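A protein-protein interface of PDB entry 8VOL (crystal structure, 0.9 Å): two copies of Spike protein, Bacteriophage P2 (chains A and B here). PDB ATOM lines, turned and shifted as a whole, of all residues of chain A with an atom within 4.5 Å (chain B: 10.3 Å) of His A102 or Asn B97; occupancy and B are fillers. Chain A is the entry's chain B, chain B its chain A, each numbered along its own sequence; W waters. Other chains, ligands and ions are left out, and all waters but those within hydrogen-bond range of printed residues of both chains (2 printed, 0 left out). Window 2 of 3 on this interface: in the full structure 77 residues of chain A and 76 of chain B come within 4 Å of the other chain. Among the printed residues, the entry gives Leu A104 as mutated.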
ATOM      1  N   HIS A  89      19.862  -4.539   6.982  1.00  0.00           N
ATOM      2  CA  HIS A  89      18.459  -4.707   6.671  1.00  0.00           C
ATOM      3  C   HIS A  89      17.760  -3.350   6.724  1.00  0.00           C
ATOM      4  O   HIS A  89      17.920  -2.607   7.696  1.00  0.00           O
ATOM      5  CB  HIS A  89      17.793  -5.679   7.642  1.00  0.00           C
ATOM      6  CG  HIS A  89      16.324  -5.627   7.513  1.00  0.00           C
ATOM      7  ND1 HIS A  89      15.524  -4.904   8.361  1.00  0.00           N
ATOM      8  CD2 HIS A  89      15.533  -6.088   6.521  1.00  0.00           C
ATOM      9  CE1 HIS A  89      14.283  -4.968   7.908  1.00  0.00           C
ATOM     10  NE2 HIS A  89      14.264  -5.676   6.790  1.00  0.00           N
ATOM     11  N   THR A  90      17.011  -3.015   5.678  1.00  0.00           N
ATOM     12  CA  THR A  90      16.274  -1.757   5.622  1.00  0.00           C
ATOM     13  C   THR A  90      14.971  -1.972   4.852  1.00  0.00           C
ATOM     14  O   THR A  90      14.766  -2.997   4.206  1.00  0.00           O
ATOM     15  CB  THR A  90      17.080  -0.619   4.972  1.00  0.00           C
ATOM     16  OG1 THR A  90      17.431  -0.993   3.644  1.00  0.00           O
ATOM     17  CG2 THR A  90      18.323  -0.247   5.784  1.00  0.00           C
ATOM     18  N   GLY A  92      11.765  -2.305   5.689  1.00  0.00           N
ATOM     19  CA  GLY A  92      10.696  -3.157   6.155  1.00  0.00           C
ATOM     20  C   GLY A  92      11.005  -3.601   7.561  1.00  0.00           C
ATOM     21  O   GLY A  92      11.837  -3.007   8.239  1.00  0.00           O
ATOM     22  N   VAL A 100       9.020  -7.439  15.805  1.00  0.00           N
ATOM     23  CA  VAL A 100       9.861  -6.599  14.966  1.00  0.00           C
ATOM     24  C   VAL A 100      11.103  -6.194  15.738  1.00  0.00           C
ATOM     25  O   VAL A 100      11.014  -5.628  16.829  1.00  0.00           O
ATOM     26  CB  VAL A 100       9.074  -5.371  14.489  1.00  0.00           C
ATOM     27  CG1 VAL A 100       9.929  -4.436  13.667  1.00  0.00           C
ATOM     28  CG2 VAL A 100       7.854  -5.788  13.668  1.00  0.00           C
ATOM     29  N   LEU A 101      12.277  -6.452  15.170  1.00  0.00           N
ATOM     30  CA  LEU A 101      13.493  -6.308  15.958  1.00  0.00           C
ATOM     31  C   LEU A 101      13.952  -4.865  16.090  1.00  0.00           C
ATOM     32  O   LEU A 101      14.539  -4.525  17.112  1.00  0.00           O
ATOM     33  CB  LEU A 101      14.595  -7.193  15.398  1.00  0.00           C
ATOM     34  CG  LEU A 101      14.304  -8.699  15.494  1.00  0.00           C
ATOM     35  CD1 LEU A 101      15.508  -9.497  15.031  1.00  0.00           C
ATOM     36  CD2 LEU A 101      13.933  -9.132  16.901  1.00  0.00           C
ATOM     37  N   HIS A 102      13.686  -3.992  15.112  1.00  0.00           N
ATOM     38  CA  HIS A 102      14.157  -2.619  15.285  1.00  0.00           C
ATOM     39  C   HIS A 102      13.356  -1.837  16.317  1.00  0.00           C
ATOM     40  O   HIS A 102      13.810  -0.773  16.736  1.00  0.00           O
ATOM     41  CB  HIS A 102      14.276  -1.865  13.957  1.00  0.00           C
ATOM     42  CG  HIS A 102      12.998  -1.315  13.438  1.00  0.00           C
ATOM     43  ND1 HIS A 102      12.098  -2.076  12.731  1.00  0.00           N
ATOM     44  CD2 HIS A 102      12.492  -0.059  13.475  1.00  0.00           C
ATOM     45  CE1 HIS A 102      11.072  -1.319  12.383  1.00  0.00           C
ATOM     46  NE2 HIS A 102      11.287  -0.093  12.821  1.00  0.00           N
ATOM     47  N   THR A 103      12.204  -2.348  16.752  1.00  0.00           N
ATOM     48  CA  THR A 103      11.402  -1.697  17.774  1.00  0.00           C
ATOM     49  C   THR A 103      11.375  -2.464  19.090  1.00  0.00           C
ATOM     50  O   THR A 103      10.658  -2.075  20.007  1.00  0.00           O
ATOM     51  CB  THR A 103       9.972  -1.456  17.281  1.00  0.00           C
ATOM     52  OG1 THR A 103       9.369  -2.693  16.890  1.00  0.00           O
ATOM     53  CG2 THR A 103       9.951  -0.484  16.108  1.00  0.00           C
ATOM     54  N   LEU A 104      12.123  -3.542  19.205  1.00  0.00           N
ATOM     55  CA  LEU A 104      12.085  -4.362  20.406  1.00  0.00           C
ATOM     56  C   LEU A 104      12.596  -3.535  21.583  1.00  0.00           C
ATOM     57  O   LEU A 104      12.151  -3.670  22.732  1.00  0.00           O
ATOM     58  CB  LEU A 104      12.934  -5.604  20.159  1.00  0.00           C
ATOM     59  CG  LEU A 104      12.575  -6.883  20.907  1.00  0.00           C
ATOM     60  CD1 LEU A 104      11.316  -7.474  20.340  1.00  0.00           C
ATOM     61  CD2 LEU A 104      13.704  -7.883  20.780  1.00  0.00           C
ATOM     62  OXT LEU A 104      13.455  -2.674  21.393  1.00  0.00           O
ATOM     63  N   LEU B  94      24.729  -6.820  12.556  1.00  0.00           N
ATOM     64  CA  LEU B  94      23.428  -6.969  11.919  1.00  0.00           C
ATOM     65  C   LEU B  94      22.623  -5.734  12.293  1.00  0.00           C
ATOM     66  O   LEU B  94      22.342  -5.511  13.478  1.00  0.00           O
ATOM     67  CB  LEU B  94      22.746  -8.234  12.420  1.00  0.00           C
ATOM     68  CG  LEU B  94      21.281  -8.428  12.043  1.00  0.00           C
ATOM     69  CD1 LEU B  94      21.089  -8.545  10.537  1.00  0.00           C
ATOM     70  CD2 LEU B  94      20.718  -9.657  12.737  1.00  0.00           C
ATOM     71  N   SER B  95      22.293  -4.917  11.298  1.00  0.00           N
ATOM     72  CA  SER B  95      21.536  -3.694  11.498  1.00  0.00           C
ATOM     73  C   SER B  95      20.157  -3.839  10.877  1.00  0.00           C
ATOM     74  O   SER B  95      20.010  -4.460   9.820  1.00  0.00           O
ATOM     75  CB  SER B  95      22.249  -2.496  10.862  1.00  0.00           C
ATOM     76  OG  SER B  95      23.500  -2.221  11.473  1.00  0.00           O
ATOM     77  N   SER B  96      19.154  -3.254  11.518  1.00  0.00           N
ATOM     78  CA  SER B  96      17.831  -3.186  10.928  1.00  0.00           C
ATOM     79  C   SER B  96      17.320  -1.766  11.096  1.00  0.00           C
ATOM     80  O   SER B  96      17.296  -1.236  12.212  1.00  0.00           O
ATOM     81  CB  SER B  96      16.845  -4.167  11.542  1.00  0.00           C
ATOM     82  OG  SER B  96      15.566  -4.001  10.948  1.00  0.00           O
ATOM     83  N   ASN B  97      16.902  -1.151   9.993  1.00  0.00           N
ATOM     84  CA  ASN B  97      16.372   0.205  10.053  1.00  0.00           C
ATOM     85  C   ASN B  97      17.347   1.165  10.716  1.00  0.00           C
ATOM     86  O   ASN B  97      16.947   2.083  11.430  1.00  0.00           O
ATOM     87  CB  ASN B  97      15.002   0.266  10.763  1.00  0.00           C
ATOM     88  CG  ASN B  97      13.889  -0.456  10.036  1.00  0.00           C
ATOM     89  OD1 ASN B  97      13.859  -1.671   9.912  1.00  0.00           O
ATOM     90  ND2 ASN B  97      12.865   0.297   9.728  1.00  0.00           N
ATOM     91  N   GLY B  98      18.640   0.951  10.482  1.00  0.00           N
ATOM     92  CA  GLY B  98      19.675   1.815  10.988  1.00  0.00           C
ATOM     93  C   GLY B  98      20.115   1.536  12.405  1.00  0.00           C
ATOM     94  O   GLY B  98      20.947   2.285  12.933  1.00  0.00           O
ATOM     95  N   LYS B  99      19.599   0.490  13.038  1.00  0.00           N
ATOM     96  CA  LYS B  99      19.926   0.151  14.417  1.00  0.00           C
ATOM     97  C   LYS B  99      20.719  -1.147  14.437  1.00  0.00           C
ATOM     98  O   LYS B  99      20.242  -2.171  13.955  1.00  0.00           O
ATOM     99  CB  LYS B  99      18.646  -0.006  15.242  1.00  0.00           C
ATOM    100  CG  LYS B  99      18.849  -0.452  16.686  1.00  0.00           C
ATOM    101  CD  LYS B  99      19.751   0.480  17.478  1.00  0.00           C
ATOM    102  CE  LYS B  99      19.410   0.439  18.959  1.00  0.00           C
ATOM    103  NZ  LYS B  99      20.464   1.072  19.794  1.00  0.00           N
ATOM    104  N   VAL B 100      21.924  -1.103  15.009  1.00  0.00           N
ATOM    105  CA  VAL B 100      22.713  -2.318  15.205  1.00  0.00           C
ATOM    106  C   VAL B 100      22.062  -3.143  16.307  1.00  0.00           C
ATOM    107  O   VAL B 100      21.830  -2.650  17.414  1.00  0.00           O
ATOM    108  CB  VAL B 100      24.169  -1.968  15.550  1.00  0.00           C
ATOM    109  CG1 VAL B 100      24.933  -3.223  15.939  1.00  0.00           C
ATOM    110  CG2 VAL B 100      24.834  -1.259  14.384  1.00  0.00           C
ATOM    111  N   LEU B 101      21.769  -4.407  16.016  1.00  0.00           N
ATOM    112  CA  LEU B 101      21.003  -5.220  16.954  1.00  0.00           C
ATOM    113  C   LEU B 101      21.860  -5.811  18.074  1.00  0.00           C
ATOM    114  O   LEU B 101      21.335  -6.075  19.162  1.00  0.00           O
ATOM    115  CB  LEU B 101      20.207  -6.275  16.192  1.00  0.00           C
ATOM    116  CG  LEU B 101      19.204  -5.678  15.190  1.00  0.00           C
ATOM    117  CD1 LEU B 101      18.419  -6.768  14.499  1.00  0.00           C
ATOM    118  CD2 LEU B 101      18.236  -4.684  15.835  1.00  0.00           C
ATOM    119  N   HIS B 102      23.154  -6.018  17.838  1.00  0.00           N
ATOM    120  CA  HIS B 102      24.088  -6.391  18.901  1.00  0.00           C
ATOM    121  C   HIS B 102      25.474  -5.877  18.517  1.00  0.00           C
ATOM    122  O   HIS B 102      26.121  -6.419  17.612  1.00  0.00           O
ATOM    123  CB  HIS B 102      24.126  -7.887  19.172  1.00  0.00           C
ATOM    124  CG  HIS B 102      24.921  -8.230  20.393  1.00  0.00           C
ATOM    125  ND1 HIS B 102      25.357  -9.506  20.669  1.00  0.00           N
ATOM    126  CD2 HIS B 102      25.386  -7.454  21.402  1.00  0.00           C
ATOM    127  CE1 HIS B 102      26.044  -9.504  21.798  1.00  0.00           C
ATOM    128  NE2 HIS B 102      26.075  -8.271  22.267  1.00  0.00           N
HETATM  129  O   HOH W   1      19.971  -1.062   8.867  1.00  0.00           O
HETATM  130  O   HOH W   2      13.053  -4.558  12.027  1.00  0.00           O
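The backbone carbonyl oxygen of His A89 sits at hydrogen-bond distance from the backbone NH of Asn B97 (2.9 Å).
O of Ser B95 is in hydrogen-bond range of N of His A89 (2.8 Å).
OD1 of Asn B97 is in hydrogen-bond range of ND1 of His A102.
OD1 of Asn B97 lies close to O of Gly A92.
The side-chain hydroxyl (OG) of Ser B96 sits at hydrogen-bond distance from a ring nitrogen (ND1) of His A89.
The backbone carbonyl oxygen of Leu B94 sits at hydrogen-bond distance from the backbone NH of Leu B101 (2.8 Å).
The side-chain hydroxyl of Ser B96 is in hydrogen-bond range of the side-chain amide oxygen of Asn B97, at 3.1 Å.
O of Leu A101 touches CD2 of Leu B101, at 3.9 Å.
His A102 touches Ser B96.
Of the printed residues of chain B, His A89 touches Ser B95 (2.8 Å), Ser B96 (2.7 Å) and Asn B97 (2.9 Å).
No residue of chain B comes within 4 Å of Val A100.
Of chain B, only Leu B101 comes within 4 Å of Leu A101.
Printed residues of chain B within 4 Å of His A102: Ser B96 and Asn B97.
No residue of chain B comes within 4 Å of Thr A103.
Leu B94 touches none of the printed residues of chain A.
Of the printed residues of chain A, Ser B95 touches His A89 (2.8 Å).
Printed residues of chain A within 4 Å of Ser B96: His A89 (2.7 Å) and His A102 (3.5 Å).
Asn B97 touches three residues of chain A.
Of the printed residues of chain A, Leu B101 touches Leu A101 (3.9 Å).
Of the 9 printed residues of chain B, 4 touch a printed residue of chain A.
Printed residues of chain B that touch a printed residue of chain A: Ser B95, Ser B96, Asn B97 and Leu B101.
Of the 8 printed residues of chain A, 4 touch a printed residue of chain B.
Among the printed residues, no Asp or Glu carboxylate lies within 4 Å of a Lys or Arg side-chain nitrogen of the other chain.
Leu A101 touches its own counterpart, Leu B101.
3 positions are printed for both chains.
Of the 7 pairs that touch across the chains among the printed residues, 1 has its exchanged pair printed and touching as well.
Water W2 lies within hydrogen-bond range of ND1 of His A102 and OG of Ser B96.
Water W1 lies within hydrogen-bond range of the backbone carbonyl oxygen of His A89 (2.8 Å), the backbone NH of Gly B98 (2.9 Å) and the backbone NH of Asn B97 (3.3 Å).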
